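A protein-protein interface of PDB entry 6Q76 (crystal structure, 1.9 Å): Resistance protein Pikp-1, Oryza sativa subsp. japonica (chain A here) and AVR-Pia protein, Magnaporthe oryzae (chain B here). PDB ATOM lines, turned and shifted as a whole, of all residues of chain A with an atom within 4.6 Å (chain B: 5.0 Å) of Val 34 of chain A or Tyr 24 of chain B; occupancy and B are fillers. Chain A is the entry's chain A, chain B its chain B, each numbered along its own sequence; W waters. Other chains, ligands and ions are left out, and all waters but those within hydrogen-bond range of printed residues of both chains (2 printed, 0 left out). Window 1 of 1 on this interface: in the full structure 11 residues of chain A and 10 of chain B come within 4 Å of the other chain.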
ATOM      1  N   SER A  19     -34.786  11.397  18.044  1.00  0.00           N
ATOM      2  CA  SER A  19     -34.361  12.788  18.092  1.00  0.00           C
ATOM      3  C   SER A  19     -33.542  13.052  19.360  1.00  0.00           C
ATOM      4  O   SER A  19     -32.560  13.774  19.351  1.00  0.00           O
ATOM      5  CB  SER A  19     -35.548  13.726  18.001  1.00  0.00           C
ATOM      6  OG  SER A  19     -35.194  15.007  18.506  1.00  0.00           O
ATOM      7  N   MET A  22     -30.117  11.310  19.162  1.00  0.00           N
ATOM      8  CA  MET A  22     -29.275  12.002  18.174  1.00  0.00           C
ATOM      9  C   MET A  22     -28.733  13.298  18.770  1.00  0.00           C
ATOM     10  O   MET A  22     -27.567  13.622  18.595  1.00  0.00           O
ATOM     11  CB  MET A  22     -30.052  12.323  16.889  1.00  0.00           C
ATOM     12  CG  MET A  22     -30.387  11.113  16.091  1.00  0.00           C
ATOM     13  SD  MET A  22     -28.974  10.509  15.150  1.00  0.00           S
ATOM     14  CE  MET A  22     -28.826  11.727  13.843  1.00  0.00           C
ATOM     15  N   ALA A  23     -29.561  14.009  19.538  1.00  0.00           N
ATOM     16  CA  ALA A  23     -29.113  15.270  20.113  1.00  0.00           C
ATOM     17  C   ALA A  23     -28.082  15.006  21.233  1.00  0.00           C
ATOM     18  O   ALA A  23     -27.083  15.722  21.371  1.00  0.00           O
ATOM     19  CB  ALA A  23     -30.311  16.065  20.612  1.00  0.00           C
ATOM     20  N   VAL A  25     -26.011  12.483  21.344  1.00  0.00           N
ATOM     21  CA  VAL A  25     -24.741  12.198  20.661  1.00  0.00           C
ATOM     22  C   VAL A  25     -24.101  13.494  20.139  1.00  0.00           C
ATOM     23  O   VAL A  25     -22.911  13.721  20.326  1.00  0.00           O
ATOM     24  CB  VAL A  25     -24.930  11.169  19.539  1.00  0.00           C
ATOM     25  CG1 VAL A  25     -23.653  10.984  18.762  1.00  0.00           C
ATOM     26  CG2 VAL A  25     -25.481   9.839  20.075  1.00  0.00           C
ATOM     27  N   ALA A  26     -24.877  14.361  19.471  1.00  0.00           N
ATOM     28  CA  ALA A  26     -24.315  15.618  18.907  1.00  0.00           C
ATOM     29  C   ALA A  26     -23.601  16.475  19.976  1.00  0.00           C
ATOM     30  O   ALA A  26     -22.577  17.211  19.709  1.00  0.00           O
ATOM     31  CB  ALA A  26     -25.443  16.385  18.258  1.00  0.00           C
ATOM     32  N   VAL A  31     -17.463  15.234  18.828  1.00  0.00           N
ATOM     33  CA  VAL A  31     -18.296  14.781  17.682  1.00  0.00           C
ATOM     34  C   VAL A  31     -18.300  15.852  16.580  1.00  0.00           C
ATOM     35  O   VAL A  31     -18.491  17.017  16.843  1.00  0.00           O
ATOM     36  CB  VAL A  31     -19.717  14.421  18.149  1.00  0.00           C
ATOM     37  CG1 VAL A  31     -20.663  14.266  16.967  1.00  0.00           C
ATOM     38  CG2 VAL A  31     -19.734  13.189  19.060  1.00  0.00           C
ATOM     39  N   ASP A  32     -18.017  15.437  15.340  1.00  0.00           N
ATOM     40  CA  ASP A  32     -18.211  16.261  14.143  1.00  0.00           C
ATOM     41  C   ASP A  32     -19.531  15.937  13.385  1.00  0.00           C
ATOM     42  O   ASP A  32     -20.131  16.864  12.819  1.00  0.00           O
ATOM     43  CB  ASP A  32     -17.061  16.099  13.159  1.00  0.00           C
ATOM     44  CG  ASP A  32     -15.737  16.629  13.678  1.00  0.00           C
ATOM     45  OD1 ASP A  32     -15.750  17.522  14.534  1.00  0.00           O
ATOM     46  OD2 ASP A  32     -14.724  16.136  13.220  1.00  0.00           O
ATOM     47  N   SER A  33     -19.915  14.666  13.261  1.00  0.00           N
ATOM     48  CA  SER A  33     -21.224  14.356  12.662  1.00  0.00           C
ATOM     49  C   SER A  33     -21.893  13.161  13.342  1.00  0.00           C
ATOM     50  O   SER A  33     -21.215  12.315  13.928  1.00  0.00           O
ATOM     51  CB  SER A  33     -21.076  14.172  11.169  1.00  0.00           C
ATOM     52  OG  SER A  33     -20.337  13.012  10.884  1.00  0.00           O
ATOM     53  N   VAL A  34     -23.237  13.107  13.234  1.00  0.00           N
ATOM     54  CA  VAL A  34     -24.104  12.061  13.755  1.00  0.00           C
ATOM     55  C   VAL A  34     -25.152  11.753  12.687  1.00  0.00           C
ATOM     56  O   VAL A  34     -25.888  12.681  12.307  1.00  0.00           O
ATOM     57  CB  VAL A  34     -24.848  12.502  15.024  1.00  0.00           C
ATOM     58  CG1 VAL A  34     -25.519  11.314  15.668  1.00  0.00           C
ATOM     59  CG2 VAL A  34     -23.948  13.232  16.001  1.00  0.00           C
ATOM     60  N   ALA A  35     -25.207  10.512  12.213  1.00  0.00           N
ATOM     61  CA  ALA A  35     -26.217  10.128  11.238  1.00  0.00           C
ATOM     62  C   ALA A  35     -27.029   8.961  11.785  1.00  0.00           C
ATOM     63  O   ALA A  35     -26.464   8.084  12.457  1.00  0.00           O
ATOM     64  CB  ALA A  35     -25.525   9.794   9.931  1.00  0.00           C
ATOM     65  N   LEU A  36     -28.336   8.930  11.477  1.00  0.00           N
ATOM     66  CA  LEU A  36     -29.141   7.710  11.591  1.00  0.00           C
ATOM     67  C   LEU A  36     -28.860   6.816  10.395  1.00  0.00           C
ATOM     68  O   LEU A  36     -29.005   7.272   9.289  1.00  0.00           O
ATOM     69  CB  LEU A  36     -30.624   8.062  11.595  1.00  0.00           C
ATOM     70  CG  LEU A  36     -31.175   8.522  12.933  1.00  0.00           C
ATOM     71  CD1 LEU A  36     -32.620   9.000  12.806  1.00  0.00           C
ATOM     72  CD2 LEU A  36     -31.063   7.407  13.957  1.00  0.00           C
ATOM     73  N   ILE A  44     -26.758   4.574  15.065  1.00  0.00           N
ATOM     74  CA  ILE A  44     -26.218   5.911  14.982  1.00  0.00           C
ATOM     75  C   ILE A  44     -24.751   5.803  14.572  1.00  0.00           C
ATOM     76  O   ILE A  44     -23.981   5.086  15.202  1.00  0.00           O
ATOM     77  CB  ILE A  44     -26.422   6.629  16.328  1.00  0.00           C
ATOM     78  CG1 ILE A  44     -27.914   6.802  16.619  1.00  0.00           C
ATOM     79  CG2 ILE A  44     -25.673   7.945  16.374  1.00  0.00           C
ATOM     80  CD1 ILE A  44     -28.230   7.411  17.973  1.00  0.00           C
ATOM     81  N   GLU A  45     -24.364   6.516  13.516  1.00  0.00           N
ATOM     82  CA  GLU A  45     -23.005   6.602  13.121  1.00  0.00           C
ATOM     83  C   GLU A  45     -22.465   7.979  13.536  1.00  0.00           C
ATOM     84  O   GLU A  45     -23.007   9.020  13.130  1.00  0.00           O
ATOM     85  CB  GLU A  45     -22.954   6.347  11.625  1.00  0.00           C
ATOM     86  CG  GLU A  45     -21.577   6.436  11.032  1.00  0.00           C
ATOM     87  CD  GLU A  45     -21.545   5.940   9.592  1.00  0.00           C
ATOM     88  OE1 GLU A  45     -22.388   5.077   9.251  1.00  0.00           O
ATOM     89  OE2 GLU A  45     -20.675   6.408   8.814  1.00  0.00           O
ATOM     90  N   PHE B   7     -24.067  23.180  15.511  1.00  0.00           N
ATOM     91  CA  PHE B   7     -24.372  22.168  14.500  1.00  0.00           C
ATOM     92  C   PHE B   7     -25.447  22.700  13.568  1.00  0.00           C
ATOM     93  O   PHE B   7     -26.295  23.487  14.019  1.00  0.00           O
ATOM     94  CB  PHE B   7     -24.912  20.887  15.159  1.00  0.00           C
ATOM     95  CG  PHE B   7     -23.871  20.065  15.866  1.00  0.00           C
ATOM     96  CD1 PHE B   7     -23.537  20.336  17.178  1.00  0.00           C
ATOM     97  CD2 PHE B   7     -23.184  19.063  15.201  1.00  0.00           C
ATOM     98  CE1 PHE B   7     -22.538  19.622  17.809  1.00  0.00           C
ATOM     99  CE2 PHE B   7     -22.206  18.343  15.839  1.00  0.00           C
ATOM    100  CZ  PHE B   7     -21.898  18.605  17.148  1.00  0.00           C
ATOM    101  N   CYS B   8     -25.446  22.172  12.332  1.00  0.00           N
ATOM    102  CA  CYS B   8     -26.563  22.207  11.396  1.00  0.00           C
ATOM    103  C   CYS B   8     -27.176  20.797  11.351  1.00  0.00           C
ATOM    104  O   CYS B   8     -26.461  19.805  11.252  1.00  0.00           O
ATOM    105  CB  CYS B   8     -26.122  22.674  10.006  1.00  0.00           C
ATOM    106  SG  CYS B   8     -25.612  24.414  10.002  1.00  0.00           S
ATOM    107  N   VAL B   9     -28.503  20.737  11.410  1.00  0.00           N
ATOM    108  CA  VAL B   9     -29.294  19.499  11.450  1.00  0.00           C
ATOM    109  C   VAL B   9     -30.068  19.389  10.135  1.00  0.00           C
ATOM    110  O   VAL B   9     -30.896  20.273   9.871  1.00  0.00           O
ATOM    111  CB  VAL B   9     -30.274  19.529  12.640  1.00  0.00           C
ATOM    112  CG1 VAL B   9     -31.036  18.225  12.802  1.00  0.00           C
ATOM    113  CG2 VAL B   9     -29.599  19.925  13.922  1.00  0.00           C
ATOM    114  N   LEU B  21     -35.452  13.094   9.782  1.00  0.00           N
ATOM    115  CA  LEU B  21     -34.139  13.522  10.313  1.00  0.00           C
ATOM    116  C   LEU B  21     -33.030  12.694   9.681  1.00  0.00           C
ATOM    117  O   LEU B  21     -33.112  11.473   9.699  1.00  0.00           O
ATOM    118  CB  LEU B  21     -34.135  13.357  11.832  1.00  0.00           C
ATOM    119  CG  LEU B  21     -32.754  13.575  12.469  1.00  0.00           C
ATOM    120  CD1 LEU B  21     -32.332  15.021  12.327  1.00  0.00           C
ATOM    121  CD2 LEU B  21     -32.752  13.174  13.928  1.00  0.00           C
ATOM    122  N   LEU B  22     -31.981  13.371   9.174  1.00  0.00           N
ATOM    123  CA  LEU B  22     -30.879  12.717   8.469  1.00  0.00           C
ATOM    124  C   LEU B  22     -29.585  12.742   9.277  1.00  0.00           C
ATOM    125  O   LEU B  22     -29.015  11.676   9.501  1.00  0.00           O
ATOM    126  CB  LEU B  22     -30.629  13.405   7.123  1.00  0.00           C
ATOM    127  CG  LEU B  22     -31.840  13.377   6.189  1.00  0.00           C
ATOM    128  CD1 LEU B  22     -31.565  14.147   4.917  1.00  0.00           C
ATOM    129  CD2 LEU B  22     -32.229  11.954   5.853  1.00  0.00           C
ATOM    130  N   MET B  23     -29.108  13.941   9.643  1.00  0.00           N
ATOM    131  CA  MET B  23     -27.742  14.072  10.197  1.00  0.00           C
ATOM    132  C   MET B  23     -27.520  15.392  10.935  1.00  0.00           C
ATOM    133  O   MET B  23     -28.083  16.436  10.583  1.00  0.00           O
ATOM    134  CB  MET B  23     -26.768  13.955   9.036  1.00  0.00           C
ATOM    135  CG  MET B  23     -25.285  14.004   9.420  1.00  0.00           C
ATOM    136  SD  MET B  23     -24.165  13.436   8.125  1.00  0.00           S
ATOM    137  CE  MET B  23     -25.169  12.232   7.284  1.00  0.00           C
ATOM    138  N   TYR B  24     -26.639  15.367  11.949  1.00  0.00           N
ATOM    139  CA  TYR B  24     -26.119  16.559  12.574  1.00  0.00           C
ATOM    140  C   TYR B  24     -24.697  16.739  12.050  1.00  0.00           C
ATOM    141  O   TYR B  24     -23.987  15.768  11.957  1.00  0.00           O
ATOM    142  CB  TYR B  24     -25.999  16.451  14.087  1.00  0.00           C
ATOM    143  CG  TYR B  24     -27.242  16.625  14.905  1.00  0.00           C
ATOM    144  CD1 TYR B  24     -28.302  15.748  14.780  1.00  0.00           C
ATOM    145  CD2 TYR B  24     -27.302  17.581  15.897  1.00  0.00           C
ATOM    146  CE1 TYR B  24     -29.425  15.875  15.573  1.00  0.00           C
ATOM    147  CE2 TYR B  24     -28.423  17.719  16.700  1.00  0.00           C
ATOM    148  CZ  TYR B  24     -29.499  16.881  16.497  1.00  0.00           C
ATOM    149  OH  TYR B  24     -30.594  16.955  17.289  1.00  0.00           O
ATOM    150  N   VAL B  25     -24.326  17.956  11.676  1.00  0.00           N
ATOM    151  CA  VAL B  25     -22.996  18.251  11.107  1.00  0.00           C
ATOM    152  C   VAL B  25     -22.480  19.475  11.852  1.00  0.00           C
ATOM    153  O   VAL B  25     -23.206  20.496  11.982  1.00  0.00           O
ATOM    154  CB  VAL B  25     -23.026  18.529   9.590  1.00  0.00           C
ATOM    155  CG1 VAL B  25     -21.619  18.773   9.037  1.00  0.00           C
ATOM    156  CG2 VAL B  25     -23.673  17.384   8.808  1.00  0.00           C
ATOM    157  N   ARG B  26     -21.236  19.385  12.316  1.00  0.00           N
ATOM    158  CA  ARG B  26     -20.678  20.440  13.140  1.00  0.00           C
ATOM    159  C   ARG B  26     -20.370  21.647  12.237  1.00  0.00           C
ATOM    160  O   ARG B  26     -19.759  21.518  11.183  1.00  0.00           O
ATOM    161  CB  ARG B  26     -19.479  19.931  13.953  1.00  0.00           C
ATOM    162  CG  ARG B  26     -18.890  21.022  14.851  1.00  0.00           C
ATOM    163  CD  ARG B  26     -17.990  20.496  15.961  1.00  0.00           C
ATOM    164  NE  ARG B  26     -16.728  20.058  15.417  1.00  0.00           N
ATOM    165  CZ  ARG B  26     -15.726  20.848  15.049  1.00  0.00           C
ATOM    166  NH1 ARG B  26     -15.804  22.162  15.200  1.00  0.00           N
ATOM    167  NH2 ARG B  26     -14.627  20.305  14.554  1.00  0.00           N
ATOM    168  N   TYR B  68     -28.660  23.785  15.531  1.00  0.00           N
ATOM    169  CA  TYR B  68     -28.815  23.235  16.874  1.00  0.00           C
ATOM    170  C   TYR B  68     -27.557  23.581  17.667  1.00  0.00           C
ATOM    171  O   TYR B  68     -26.400  23.453  17.200  1.00  0.00           O
ATOM    172  CB  TYR B  68     -29.100  21.736  16.794  1.00  0.00           C
ATOM    173  CG  TYR B  68     -28.925  20.994  18.091  1.00  0.00           C
ATOM    174  CD1 TYR B  68     -27.655  20.628  18.523  1.00  0.00           C
ATOM    175  CD2 TYR B  68     -30.009  20.688  18.891  1.00  0.00           C
ATOM    176  CE1 TYR B  68     -27.475  19.929  19.703  1.00  0.00           C
ATOM    177  CE2 TYR B  68     -29.846  20.003  20.088  1.00  0.00           C
ATOM    178  CZ  TYR B  68     -28.574  19.626  20.488  1.00  0.00           C
ATOM    179  OH  TYR B  68     -28.374  18.961  21.653  1.00  0.00           O
ATOM    180  OXT TYR B  68     -27.695  24.055  18.765  1.00  0.00           O
HETATM  181  O   HOH W   1     -13.029  18.317  13.429  1.00  0.00           O
HETATM  182  O   HOH W   2     -32.590  15.240  16.926  1.00  0.00           O
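The backbone carbonyl oxygen (O) of Ala 23 of chain A lies within hydrogen-bond range of the side-chain hydroxyl (OH) of Tyr 68 of chain B.
OD1 of Asp 32 of chain A lies within salt-bridge range of NE of Arg 26 of chain B (2.9 Å).
O of Val 34 of chain A is in hydrogen-bond range of N of Tyr 24 of chain B, at 2.8 Å.
The backbone carbonyl oxygen (O) of Leu 22 of chain B is in hydrogen-bond range of the backbone NH (N) of Leu 36 of chain A, 3.5 Å away.
Ala 23 of chain A touches Tyr 24 of chain B (CB to OH, 3.5 Å).
CZ of Phe 7 of chain B touches O of Ala 26 of chain A, 3.0 Å away.
Ala 26 of chain A touches Tyr 24 of chain B (CB to CD2, 3.2 Å).
CD of Arg 26 of chain B touches O of Val 31 of chain A, 3.6 Å away.
CE2 of Phe 7 of chain B touches O of Asp 32 of chain A (3.95 Å).
O of Asp 32 of chain A touches CA of Val 25 of chain B, 3.6 Å away.
CA of Ser 33 of chain A touches O of Tyr 24 of chain B, at 3.2 Å.
CA of Met 23 of chain B touches O of Val 34 of chain A (3.1 Å).
Ala 35 of chain A touches Leu 22 of chain B.
Ala 35 of chain A touches Met 23 of chain B.
Water W2 lies within hydrogen-bond range of OH of Tyr 24 of chain B (2.7 Å) and O of Ser 19 of chain A (2.8 Å).
Water W1 lies within hydrogen-bond range of OD2 of Asp 32 of chain A (2.8 Å) and NH2 of Arg 26 of chain B (2.8 Å).
Of chain B, only Met 23 and Tyr 24 come within 4 Å of Val 34 of chain A.
Of the printed residues of chain A, Leu 21 of chain B touches Met 22.
Of the printed residues of chain A, Leu 22 of chain B touches Ala 35 (3.6 Å) and Leu 36 (3.5 Å).
Of the printed residues of chain A, Met 23 of chain B touches Val 34 and Ala 35.
Tyr 24 of chain B touches just these residues of chain A: Met 22, Ala 23, Ala 26, Ser 33 and Val 34.
Of the printed residues of chain A, Val 25 of chain B touches Asp 32 (3.6 Å).
Of the printed residues of chain A, Tyr 68 of chain B touches Ala 23 (3.5 Å).
The nearest residue of chain B that does not touch Val 34 of chain A is Leu 22 of chain B (4.3 Å).
The nearest printed residue of chain B that does not touch Val 31 of chain A is Tyr 24 of chain B (6.2 Å).
The backbone NH of Ala 35 of chain A is in hydrogen-bond range of the backbone carbonyl oxygen of Glu 45 of chain A, at 2.8 Å.
The backbone carbonyl oxygen of Phe 7 of chain B lies within hydrogen-bond range of the backbone NH of Tyr 68 of chain B (2.8 Å).
O of Val 25 of chain B sits at hydrogen-bond distance from N of Cys 8 of chain B, at 2.8 Å.
Of the 13 printed residues of chain A, 9 touch a printed residue of chain B.
Printed residues of chain A that touch a printed residue of chain B: Met 22, Ala 23, Ala 26, Val 31, Asp 32, Ser 33, Val 34, Ala 35 and Leu 36.
Printed residues of chain B that touch a printed residue of chain A: Phe 7, Leu 21, Leu 22, Met 23, Tyr 24, Val 25, Arg 26 and Tyr 68.
Hydrophobic or aromatic side chains of chain B that line the printed part of chain A: Phe 7, Leu 21, Met 23, Tyr 24 and Tyr 68.
Among the printed residues, Asp or Glu carboxylates within 4 Å of a Lys or Arg side-chain nitrogen of the other chain: Asp 32 of chain A with Arg 26 of chain B.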
